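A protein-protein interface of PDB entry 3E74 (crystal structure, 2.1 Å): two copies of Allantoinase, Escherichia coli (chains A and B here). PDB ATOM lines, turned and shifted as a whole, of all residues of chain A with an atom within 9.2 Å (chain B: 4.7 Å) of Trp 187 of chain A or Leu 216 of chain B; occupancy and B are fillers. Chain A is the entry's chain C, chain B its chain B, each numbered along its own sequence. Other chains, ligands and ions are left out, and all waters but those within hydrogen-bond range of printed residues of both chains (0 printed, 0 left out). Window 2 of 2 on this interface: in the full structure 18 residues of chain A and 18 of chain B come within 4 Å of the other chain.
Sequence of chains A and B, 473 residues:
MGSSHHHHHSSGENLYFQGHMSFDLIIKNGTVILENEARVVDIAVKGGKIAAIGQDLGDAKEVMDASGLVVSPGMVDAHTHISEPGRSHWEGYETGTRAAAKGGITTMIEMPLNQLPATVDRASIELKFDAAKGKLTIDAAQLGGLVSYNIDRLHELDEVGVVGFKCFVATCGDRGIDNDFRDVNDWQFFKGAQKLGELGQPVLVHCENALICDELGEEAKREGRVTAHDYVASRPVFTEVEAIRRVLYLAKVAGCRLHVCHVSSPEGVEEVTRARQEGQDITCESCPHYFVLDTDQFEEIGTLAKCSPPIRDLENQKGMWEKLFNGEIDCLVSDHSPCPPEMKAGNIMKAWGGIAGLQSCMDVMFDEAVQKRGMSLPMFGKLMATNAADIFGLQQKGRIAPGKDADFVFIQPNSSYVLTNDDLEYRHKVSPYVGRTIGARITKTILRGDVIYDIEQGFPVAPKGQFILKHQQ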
ATOM      1  N   LEU A 146     -22.977  13.671   4.251  1.00  0.00           N
ATOM      2  CA  LEU A 146     -22.908  15.083   4.567  1.00  0.00           C
ATOM      3  C   LEU A 146     -23.704  15.697   3.438  1.00  0.00           C
ATOM      4  O   LEU A 146     -23.216  15.779   2.317  1.00  0.00           O
ATOM      5  CB  LEU A 146     -21.467  15.608   4.521  1.00  0.00           C
ATOM      6  CG  LEU A 146     -21.355  17.126   4.303  1.00  0.00           C
ATOM      7  CD1 LEU A 146     -22.075  17.855   5.407  1.00  0.00           C
ATOM      8  CD2 LEU A 146     -19.909  17.544   4.265  1.00  0.00           C
ATOM      9  N   VAL A 147     -24.943  16.082   3.715  1.00  0.00           N
ATOM     10  CA  VAL A 147     -25.762  16.698   2.685  1.00  0.00           C
ATOM     11  C   VAL A 147     -26.069  18.150   3.057  1.00  0.00           C
ATOM     12  O   VAL A 147     -25.810  18.583   4.181  1.00  0.00           O
ATOM     13  CB  VAL A 147     -27.058  15.890   2.447  1.00  0.00           C
ATOM     14  CG1 VAL A 147     -26.697  14.542   1.819  1.00  0.00           C
ATOM     15  CG2 VAL A 147     -27.802  15.688   3.748  1.00  0.00           C
ATOM     16  N   SER A 148     -26.608  18.905   2.111  1.00  0.00           N
ATOM     17  CA  SER A 148     -26.887  20.319   2.342  1.00  0.00           C
ATOM     18  C   SER A 148     -27.882  20.612   3.442  1.00  0.00           C
ATOM     19  O   SER A 148     -27.968  21.738   3.914  1.00  0.00           O
ATOM     20  CB  SER A 148     -27.409  20.952   1.071  1.00  0.00           C
ATOM     21  OG  SER A 148     -28.666  20.387   0.781  1.00  0.00           O
ATOM     22  N   ILE A 151     -26.217  19.501   8.227  1.00  0.00           N
ATOM     23  CA  ILE A 151     -25.011  19.944   8.920  1.00  0.00           C
ATOM     24  C   ILE A 151     -25.231  20.070  10.423  1.00  0.00           C
ATOM     25  O   ILE A 151     -24.281  20.070  11.207  1.00  0.00           O
ATOM     26  CB  ILE A 151     -24.500  21.284   8.336  1.00  0.00           C
ATOM     27  CG1 ILE A 151     -24.236  21.107   6.832  1.00  0.00           C
ATOM     28  CG2 ILE A 151     -23.215  21.720   9.042  1.00  0.00           C
ATOM     29  CD1 ILE A 151     -23.554  22.288   6.153  1.00  0.00           C
ATOM     30  N   VAL A 169     -19.430  17.333  -4.166  1.00  0.00           N
ATOM     31  CA  VAL A 169     -19.318  18.777  -4.294  1.00  0.00           C
ATOM     32  C   VAL A 169     -19.776  19.266  -5.657  1.00  0.00           C
ATOM     33  O   VAL A 169     -20.696  20.083  -5.751  1.00  0.00           O
ATOM     34  CB  VAL A 169     -17.872  19.227  -4.064  1.00  0.00           C
ATOM     35  CG1 VAL A 169     -17.459  18.917  -2.636  1.00  0.00           C
ATOM     36  CG2 VAL A 169     -16.946  18.519  -5.064  1.00  0.00           C
ATOM     37  N   VAL A 184     -23.527  19.114  -1.980  1.00  0.00           N
ATOM     38  CA  VAL A 184     -23.363  20.331  -1.197  1.00  0.00           C
ATOM     39  C   VAL A 184     -22.609  21.387  -2.000  1.00  0.00           C
ATOM     40  O   VAL A 184     -21.801  21.043  -2.864  1.00  0.00           O
ATOM     41  CB  VAL A 184     -22.602  20.039   0.110  1.00  0.00           C
ATOM     42  CG1 VAL A 184     -23.462  19.174   1.019  1.00  0.00           C
ATOM     43  CG2 VAL A 184     -21.284  19.341  -0.190  1.00  0.00           C
ATOM     44  N   ASN A 185     -22.877  22.667  -1.748  1.00  0.00           N
ATOM     45  CA  ASN A 185     -22.142  23.697  -2.486  1.00  0.00           C
ATOM     46  C   ASN A 185     -20.874  24.001  -1.700  1.00  0.00           C
ATOM     47  O   ASN A 185     -20.707  23.468  -0.596  1.00  0.00           O
ATOM     48  CB  ASN A 185     -22.979  24.960  -2.700  1.00  0.00           C
ATOM     49  CG  ASN A 185     -23.523  25.540  -1.418  1.00  0.00           C
ATOM     50  OD1 ASN A 185     -22.839  25.573  -0.393  1.00  0.00           O
ATOM     51  ND2 ASN A 185     -24.764  26.040  -1.477  1.00  0.00           N
ATOM     52  N   ASP A 186     -19.981  24.828  -2.253  1.00  0.00           N
ATOM     53  CA  ASP A 186     -18.722  25.142  -1.572  1.00  0.00           C
ATOM     54  C   ASP A 186     -18.938  25.561  -0.128  1.00  0.00           C
ATOM     55  O   ASP A 186     -18.175  25.173   0.745  1.00  0.00           O
ATOM     56  CB  ASP A 186     -17.938  26.246  -2.305  1.00  0.00           C
ATOM     57  CG  ASP A 186     -17.525  25.839  -3.713  1.00  0.00           C
ATOM     58  OD1 ASP A 186     -17.273  24.637  -3.944  1.00  0.00           O
ATOM     59  OD2 ASP A 186     -17.442  26.721  -4.600  1.00  0.00           O
ATOM     60  N   TRP A 187     -19.984  26.344   0.124  1.00  0.00           N
ATOM     61  CA  TRP A 187     -20.266  26.800   1.493  1.00  0.00           C
ATOM     62  C   TRP A 187     -20.674  25.647   2.410  1.00  0.00           C
ATOM     63  O   TRP A 187     -20.156  25.504   3.515  1.00  0.00           O
ATOM     64  CB  TRP A 187     -21.371  27.881   1.502  1.00  0.00           C
ATOM     65  CG  TRP A 187     -21.936  28.165   2.867  1.00  0.00           C
ATOM     66  CD1 TRP A 187     -23.201  27.882   3.304  1.00  0.00           C
ATOM     67  CD2 TRP A 187     -21.246  28.736   3.990  1.00  0.00           C
ATOM     68  NE1 TRP A 187     -23.341  28.239   4.625  1.00  0.00           N
ATOM     69  CE2 TRP A 187     -22.160  28.764   5.072  1.00  0.00           C
ATOM     70  CE3 TRP A 187     -19.946  29.227   4.188  1.00  0.00           C
ATOM     71  CZ2 TRP A 187     -21.815  29.262   6.335  1.00  0.00           C
ATOM     72  CZ3 TRP A 187     -19.605  29.723   5.444  1.00  0.00           C
ATOM     73  CH2 TRP A 187     -20.540  29.736   6.501  1.00  0.00           C
ATOM     74  N   GLN A 188     -21.614  24.834   1.954  1.00  0.00           N
ATOM     75  CA  GLN A 188     -22.068  23.713   2.758  1.00  0.00           C
ATOM     76  C   GLN A 188     -20.910  22.758   2.989  1.00  0.00           C
ATOM     77  O   GLN A 188     -20.783  22.178   4.066  1.00  0.00           O
ATOM     78  CB  GLN A 188     -23.255  23.038   2.073  1.00  0.00           C
ATOM     79  CG  GLN A 188     -24.479  23.969   2.061  1.00  0.00           C
ATOM     80  CD  GLN A 188     -25.493  23.660   0.967  1.00  0.00           C
ATOM     81  OE1 GLN A 188     -25.191  22.984  -0.022  1.00  0.00           O
ATOM     82  NE2 GLN A 188     -26.694  24.172   1.133  1.00  0.00           N
ATOM     83  N   PHE A 189     -20.042  22.623   1.994  1.00  0.00           N
ATOM     84  CA  PHE A 189     -18.878  21.763   2.145  1.00  0.00           C
ATOM     85  C   PHE A 189     -17.910  22.331   3.183  1.00  0.00           C
ATOM     86  O   PHE A 189     -17.446  21.611   4.056  1.00  0.00           O
ATOM     87  CB  PHE A 189     -18.123  21.584   0.829  1.00  0.00           C
ATOM     88  CG  PHE A 189     -16.933  20.698   0.964  1.00  0.00           C
ATOM     89  CD1 PHE A 189     -17.097  19.320   1.143  1.00  0.00           C
ATOM     90  CD2 PHE A 189     -15.653  21.240   1.021  1.00  0.00           C
ATOM     91  CE1 PHE A 189     -15.998  18.503   1.385  1.00  0.00           C
ATOM     92  CE2 PHE A 189     -14.549  20.444   1.261  1.00  0.00           C
ATOM     93  CZ  PHE A 189     -14.718  19.063   1.446  1.00  0.00           C
ATOM     94  N   PHE A 190     -17.599  23.623   3.094  1.00  0.00           N
ATOM     95  CA  PHE A 190     -16.688  24.225   4.063  1.00  0.00           C
ATOM     96  C   PHE A 190     -17.284  24.158   5.480  1.00  0.00           C
ATOM     97  O   PHE A 190     -16.612  23.762   6.443  1.00  0.00           O
ATOM     98  CB  PHE A 190     -16.391  25.685   3.695  1.00  0.00           C
ATOM     99  CG  PHE A 190     -15.575  26.424   4.736  1.00  0.00           C
ATOM    100  CD1 PHE A 190     -14.205  26.207   4.859  1.00  0.00           C
ATOM    101  CD2 PHE A 190     -16.184  27.334   5.596  1.00  0.00           C
ATOM    102  CE1 PHE A 190     -13.458  26.887   5.820  1.00  0.00           C
ATOM    103  CE2 PHE A 190     -15.445  28.018   6.560  1.00  0.00           C
ATOM    104  CZ  PHE A 190     -14.083  27.793   6.674  1.00  0.00           C
ATOM    105  N   LYS A 191     -18.552  24.543   5.585  1.00  0.00           N
ATOM    106  CA  LYS A 191     -19.264  24.560   6.851  1.00  0.00           C
ATOM    107  C   LYS A 191     -19.337  23.143   7.422  1.00  0.00           C
ATOM    108  O   LYS A 191     -19.051  22.918   8.603  1.00  0.00           O
ATOM    109  CB  LYS A 191     -20.661  25.111   6.613  1.00  0.00           C
ATOM    110  CG  LYS A 191     -21.426  25.460   7.864  1.00  0.00           C
ATOM    111  CD  LYS A 191     -21.005  26.827   8.407  1.00  0.00           C
ATOM    112  CE  LYS A 191     -22.040  27.348   9.415  1.00  0.00           C
ATOM    113  NZ  LYS A 191     -23.429  27.338   8.841  1.00  0.00           N
ATOM    114  N   GLY A 192     -19.707  22.186   6.575  1.00  0.00           N
ATOM    115  CA  GLY A 192     -19.785  20.801   7.011  1.00  0.00           C
ATOM    116  C   GLY A 192     -18.436  20.222   7.425  1.00  0.00           C
ATOM    117  O   GLY A 192     -18.333  19.601   8.483  1.00  0.00           O
ATOM    118  N   ALA A 193     -17.404  20.425   6.603  1.00  0.00           N
ATOM    119  CA  ALA A 193     -16.065  19.909   6.901  1.00  0.00           C
ATOM    120  C   ALA A 193     -15.520  20.456   8.214  1.00  0.00           C
ATOM    121  O   ALA A 193     -14.877  19.746   8.987  1.00  0.00           O
ATOM    122  CB  ALA A 193     -15.112  20.262   5.776  1.00  0.00           C
ATOM    123  N   GLN A 194     -15.759  21.743   8.443  1.00  0.00           N
ATOM    124  CA  GLN A 194     -15.296  22.400   9.655  1.00  0.00           C
ATOM    125  C   GLN A 194     -15.903  21.691  10.877  1.00  0.00           C
ATOM    126  O   GLN A 194     -15.217  21.417  11.855  1.00  0.00           O
ATOM    127  CB  GLN A 194     -15.706  23.872   9.604  1.00  0.00           C
ATOM    128  CG  GLN A 194     -14.987  24.762  10.571  1.00  0.00           C
ATOM    129  CD  GLN A 194     -15.208  26.234  10.248  1.00  0.00           C
ATOM    130  OE1 GLN A 194     -14.256  27.019  10.183  1.00  0.00           O
ATOM    131  NE2 GLN A 194     -16.463  26.611  10.040  1.00  0.00           N
ATOM    132  N   LYS A 195     -17.192  21.374  10.801  1.00  0.00           N
ATOM    133  CA  LYS A 195     -17.866  20.662  11.890  1.00  0.00           C
ATOM    134  C   LYS A 195     -17.271  19.260  12.063  1.00  0.00           C
ATOM    135  O   LYS A 195     -16.969  18.842  13.185  1.00  0.00           O
ATOM    136  CB  LYS A 195     -19.376  20.567  11.608  1.00  0.00           C
ATOM    137  CG  LYS A 195     -20.157  19.560  12.498  1.00  0.00           C
ATOM    138  CD  LYS A 195     -20.585  20.135  13.848  1.00  0.00           C
ATOM    139  CE  LYS A 195     -21.559  19.193  14.596  1.00  0.00           C
ATOM    140  NZ  LYS A 195     -22.952  19.043  14.008  1.00  0.00           N
ATOM    141  N   ARG A 246      -9.790  21.874  -5.620  1.00  0.00           N
ATOM    142  CA  ARG A 246     -10.780  22.651  -4.902  1.00  0.00           C
ATOM    143  C   ARG A 246     -11.057  22.054  -3.519  1.00  0.00           C
ATOM    144  O   ARG A 246     -10.936  22.741  -2.510  1.00  0.00           O
ATOM    145  CB  ARG A 246     -12.068  22.679  -5.719  1.00  0.00           C
ATOM    146  CG  ARG A 246     -13.305  22.736  -4.888  1.00  0.00           C
ATOM    147  CD  ARG A 246     -13.859  24.116  -4.906  1.00  0.00           C
ATOM    148  NE  ARG A 246     -14.290  24.462  -6.252  1.00  0.00           N
ATOM    149  CZ  ARG A 246     -15.109  23.720  -6.986  1.00  0.00           C
ATOM    150  NH1 ARG A 246     -15.583  22.579  -6.507  1.00  0.00           N
ATOM    151  NH2 ARG A 246     -15.481  24.131  -8.194  1.00  0.00           N
ATOM    152  N   LEU A 250     -10.216  23.673   0.460  1.00  0.00           N
ATOM    153  CA  LEU A 250     -11.288  23.924   1.415  1.00  0.00           C
ATOM    154  C   LEU A 250     -11.206  23.041   2.656  1.00  0.00           C
ATOM    155  O   LEU A 250     -11.489  23.509   3.764  1.00  0.00           O
ATOM    156  CB  LEU A 250     -12.649  23.731   0.750  1.00  0.00           C
ATOM    157  CG  LEU A 250     -12.947  24.732  -0.372  1.00  0.00           C
ATOM    158  CD1 LEU A 250     -14.269  24.400  -1.040  1.00  0.00           C
ATOM    159  CD2 LEU A 250     -12.977  26.142   0.209  1.00  0.00           C
ATOM    160  N   VAL A 253      -8.450  24.425   4.852  1.00  0.00           N
ATOM    161  CA  VAL A 253      -8.889  25.606   5.583  1.00  0.00           C
ATOM    162  C   VAL A 253      -9.879  25.239   6.681  1.00  0.00           C
ATOM    163  O   VAL A 253      -9.874  25.839   7.755  1.00  0.00           O
ATOM    164  CB  VAL A 253      -9.567  26.653   4.667  1.00  0.00           C
ATOM    165  CG1 VAL A 253      -9.751  27.965   5.448  1.00  0.00           C
ATOM    166  CG2 VAL A 253      -8.732  26.899   3.438  1.00  0.00           C
ATOM    167  N   ALA A 254     -10.722  24.245   6.419  1.00  0.00           N
ATOM    168  CA  ALA A 254     -11.719  23.852   7.399  1.00  0.00           C
ATOM    169  C   ALA A 254     -11.117  23.028   8.523  1.00  0.00           C
ATOM    170  O   ALA A 254     -11.759  22.826   9.545  1.00  0.00           O
ATOM    171  CB  ALA A 254     -12.853  23.079   6.722  1.00  0.00           C
ATOM    172  N   LEU B 211     -19.974  32.740  -2.929  1.00  0.00           N
ATOM    173  CA  LEU B 211     -20.884  31.979  -2.098  1.00  0.00           C
ATOM    174  C   LEU B 211     -20.457  32.012  -0.647  1.00  0.00           C
ATOM    175  O   LEU B 211     -21.250  32.364   0.232  1.00  0.00           O
ATOM    176  CB  LEU B 211     -20.960  30.532  -2.572  1.00  0.00           C
ATOM    177  CG  LEU B 211     -21.804  29.644  -1.648  1.00  0.00           C
ATOM    178  CD1 LEU B 211     -23.215  30.199  -1.525  1.00  0.00           C
ATOM    179  CD2 LEU B 211     -21.837  28.238  -2.207  1.00  0.00           C
ATOM    180  N   ILE B 212     -19.206  31.644  -0.392  1.00  0.00           N
ATOM    181  CA  ILE B 212     -18.712  31.629   0.973  1.00  0.00           C
ATOM    182  C   ILE B 212     -18.719  33.027   1.569  1.00  0.00           C
ATOM    183  O   ILE B 212     -19.025  33.201   2.750  1.00  0.00           O
ATOM    184  CB  ILE B 212     -17.285  31.035   1.056  1.00  0.00           C
ATOM    185  CG1 ILE B 212     -17.302  29.569   0.587  1.00  0.00           C
ATOM    186  CG2 ILE B 212     -16.766  31.124   2.492  1.00  0.00           C
ATOM    187  CD1 ILE B 212     -15.946  28.854   0.700  1.00  0.00           C
ATOM    188  N   CYS B 213     -18.380  34.033   0.767  1.00  0.00           N
ATOM    189  CA  CYS B 213     -18.383  35.395   1.288  1.00  0.00           C
ATOM    190  C   CYS B 213     -19.802  35.811   1.701  1.00  0.00           C
ATOM    191  O   CYS B 213     -20.007  36.304   2.813  1.00  0.00           O
ATOM    192  CB  CYS B 213     -17.814  36.378   0.252  1.00  0.00           C
ATOM    193  SG  CYS B 213     -16.007  36.281   0.096  1.00  0.00           S
ATOM    194  N   ASP B 214     -20.770  35.587   0.814  1.00  0.00           N
ATOM    195  CA  ASP B 214     -22.159  35.950   1.085  1.00  0.00           C
ATOM    196  C   ASP B 214     -22.681  35.280   2.347  1.00  0.00           C
ATOM    197  O   ASP B 214     -23.272  35.936   3.207  1.00  0.00           O
ATOM    198  CB  ASP B 214     -23.072  35.572  -0.095  1.00  0.00           C
ATOM    199  CG  ASP B 214     -22.730  36.327  -1.378  1.00  0.00           C
ATOM    200  OD1 ASP B 214     -22.442  37.540  -1.304  1.00  0.00           O
ATOM    201  OD2 ASP B 214     -22.764  35.715  -2.469  1.00  0.00           O
ATOM    202  N   GLU B 215     -22.455  33.973   2.452  1.00  0.00           N
ATOM    203  CA  GLU B 215     -22.904  33.203   3.602  1.00  0.00           C
ATOM    204  C   GLU B 215     -22.269  33.701   4.880  1.00  0.00           C
ATOM    205  O   GLU B 215     -22.962  33.871   5.885  1.00  0.00           O
ATOM    206  CB  GLU B 215     -22.587  31.728   3.403  1.00  0.00           C
ATOM    207  CG  GLU B 215     -23.460  31.073   2.357  1.00  0.00           C
ATOM    208  CD  GLU B 215     -24.935  31.035   2.765  1.00  0.00           C
ATOM    209  OE1 GLU B 215     -25.219  30.941   3.983  1.00  0.00           O
ATOM    210  OE2 GLU B 215     -25.803  31.082   1.865  1.00  0.00           O
ATOM    211  N   LEU B 216     -20.957  33.934   4.852  1.00  0.00           N
ATOM    212  CA  LEU B 216     -20.266  34.444   6.032  1.00  0.00           C
ATOM    213  C   LEU B 216     -20.807  35.829   6.379  1.00  0.00           C
ATOM    214  O   LEU B 216     -20.908  36.193   7.553  1.00  0.00           O
ATOM    215  CB  LEU B 216     -18.763  34.526   5.782  1.00  0.00           C
ATOM    216  CG  LEU B 216     -18.031  33.187   5.722  1.00  0.00           C
ATOM    217  CD1 LEU B 216     -16.584  33.420   5.310  1.00  0.00           C
ATOM    218  CD2 LEU B 216     -18.104  32.499   7.088  1.00  0.00           C
ATOM    219  N   GLY B 217     -21.153  36.598   5.349  1.00  0.00           N
ATOM    220  CA  GLY B 217     -21.700  37.922   5.578  1.00  0.00           C
ATOM    221  C   GLY B 217     -23.056  37.810   6.257  1.00  0.00           C
ATOM    222  O   GLY B 217     -23.340  38.519   7.227  1.00  0.00           O
ATOM    223  N   GLU B 218     -23.894  36.907   5.749  1.00  0.00           N
ATOM    224  CA  GLU B 218     -25.223  36.691   6.311  1.00  0.00           C
ATOM    225  C   GLU B 218     -25.104  36.177   7.738  1.00  0.00           C
ATOM    226  O   GLU B 218     -25.998  36.367   8.557  1.00  0.00           O
ATOM    227  CB  GLU B 218     -26.001  35.675   5.475  1.00  0.00           C
ATOM    228  CG  GLU B 218     -27.347  36.179   5.033  1.00  0.00           C
ATOM    229  CD  GLU B 218     -27.233  37.329   4.046  1.00  0.00           C
ATOM    230  OE1 GLU B 218     -26.974  37.066   2.849  1.00  0.00           O
ATOM    231  OE2 GLU B 218     -27.393  38.498   4.467  1.00  0.00           O
ATOM    232  N   GLU B 219     -23.990  35.522   8.034  1.00  0.00           N
ATOM    233  CA  GLU B 219     -23.760  34.984   9.366  1.00  0.00           C
ATOM    234  C   GLU B 219     -23.342  36.085  10.346  1.00  0.00           C
ATOM    235  O   GLU B 219     -23.654  36.021  11.535  1.00  0.00           O
ATOM    236  CB  GLU B 219     -22.688  33.906   9.298  1.00  0.00           C
ATOM    237  CG  GLU B 219     -22.533  33.105  10.558  1.00  0.00           C
ATOM    238  CD  GLU B 219     -21.485  32.027  10.408  1.00  0.00           C
ATOM    239  OE1 GLU B 219     -20.281  32.352  10.513  1.00  0.00           O
ATOM    240  OE2 GLU B 219     -21.866  30.860  10.166  1.00  0.00           O
ATOM    241  N   ALA B 220     -22.625  37.089   9.852  1.00  0.00           N
ATOM    242  CA  ALA B 220     -22.202  38.196  10.703  1.00  0.00           C
ATOM    243  C   ALA B 220     -23.462  38.992  10.999  1.00  0.00           C
ATOM    244  O   ALA B 220     -23.649  39.501  12.099  1.00  0.00           O
ATOM    245  CB  ALA B 220     -21.188  39.069   9.977  1.00  0.00           C
ATOM    246  N   ALA B 233     -13.585  40.126   7.936  1.00  0.00           N
ATOM    247  CA  ALA B 233     -13.543  38.734   8.366  1.00  0.00           C
ATOM    248  C   ALA B 233     -14.499  37.831   7.588  1.00  0.00           C
ATOM    249  O   ALA B 233     -14.257  36.628   7.478  1.00  0.00           O
ATOM    250  CB  ALA B 233     -13.836  38.643   9.862  1.00  0.00           C
ATOM    251  N   SER B 234     -15.586  38.396   7.061  1.00  0.00           N
ATOM    252  CA  SER B 234     -16.542  37.603   6.282  1.00  0.00           C
ATOM    253  C   SER B 234     -16.044  37.430   4.841  1.00  0.00           C
ATOM    254  O   SER B 234     -16.669  36.753   4.035  1.00  0.00           O
ATOM    255  CB  SER B 234     -17.927  38.265   6.279  1.00  0.00           C
ATOM    256  OG  SER B 234     -17.939  39.440   5.489  1.00  0.00           O
ATOM    257  N   PRO B 236     -12.629  36.410   4.175  1.00  0.00           N
ATOM    258  CA  PRO B 236     -11.270  35.961   4.493  1.00  0.00           C
ATOM    259  C   PRO B 236     -10.401  35.638   3.278  1.00  0.00           C
ATOM    260  O   PRO B 236     -10.901  35.340   2.188  1.00  0.00           O
ATOM    261  CB  PRO B 236     -11.515  34.751   5.395  1.00  0.00           C
ATOM    262  CG  PRO B 236     -12.792  34.190   4.844  1.00  0.00           C
ATOM    263  CD  PRO B 236     -13.630  35.418   4.612  1.00  0.00           C
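Printed residues of chain B within 4 Å of Asn 185 of chain A: Leu 211 (3.3 Å).
Of the printed residues of chain B, Asp 186 of chain A touches Leu 211.
Of chain B, only Leu 211, Glu 215 and Leu 216 come within 4 Å of Trp 187 of chain A.
Of the printed residues of chain B, Lys 191 of chain A touches Glu 219.
Val 253 of chain A touches none of the printed residues of chain B.
Printed residues of chain A within 4 Å of Leu 211 of chain B: Asn 185 (3.3 Å), Asp 186 (3.9 Å) and Trp 187 (3.5 Å).
No residue of chain A comes within 4 Å of Ile 212 of chain B.
Of chain A, only Trp 187 comes within 4 Å of Glu 215 of chain B.
Of chain A, only Trp 187 (3.6 Å) comes within 4 Å of Leu 216 of chain B.
No residue of chain A comes within 4 Å of Gly 217 of chain B.
Glu 219 of chain B touches just one residue of chain A: Lys 191 (3.6 Å).
Ala 233 of chain B touches none of the printed residues of chain A.
The nearest printed residue of chain B that does not touch Trp 187 of chain A is Glu 219 of chain B (4.1 Å).
The nearest residue of chain A that does not touch Leu 216 of chain B is Phe 190 of chain A (5.2 Å).
OE1 of Glu 215 of chain B sits at hydrogen-bond distance from NE1 of Trp 187 of chain A, at 3.4 Å.
Hydrophobic or aromatic side chains of chain A that line the printed part of chain B: Trp 187.
Printed residues of chain B that touch a printed residue of chain A: Leu 211, Glu 215, Leu 216 and Glu 219.
Among the printed residues, 6 pairs touch across the chains.
Among the printed residues, no Asp or Glu carboxylate lies within 4 Å of a Lys or Arg side-chain nitrogen of the other chain.
Among the printed residues, pairs that only touch across the chains: Asn 185 of chain A with Leu 211 of chain B, Trp 187 of chain A with Leu 211 of chain B, Trp 187 of chain A with Leu 216 of chain B, Lys 191 of chain A with Glu 219 of chain B and Asp 186 of chain A with Leu 211 of chain B.
No position is printed for both chains.
Of the 6 pairs that touch across the chains among the printed residues, none has its exchanged pair printed and touching as well.
N of Trp 187 of chain A lies within hydrogen-bond range of OD1 of Asn 185 of chain A.
OD1 of Asn 185 of chain A lies within hydrogen-bond range of N of Gln 188 of chain A, 2.7 Å away.
The guanidinium group (NH1) of Arg 246 of chain A is in salt-bridge range of the side-chain carboxylate (OD1) of Asp 186 of chain A, 3.7 Å away.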
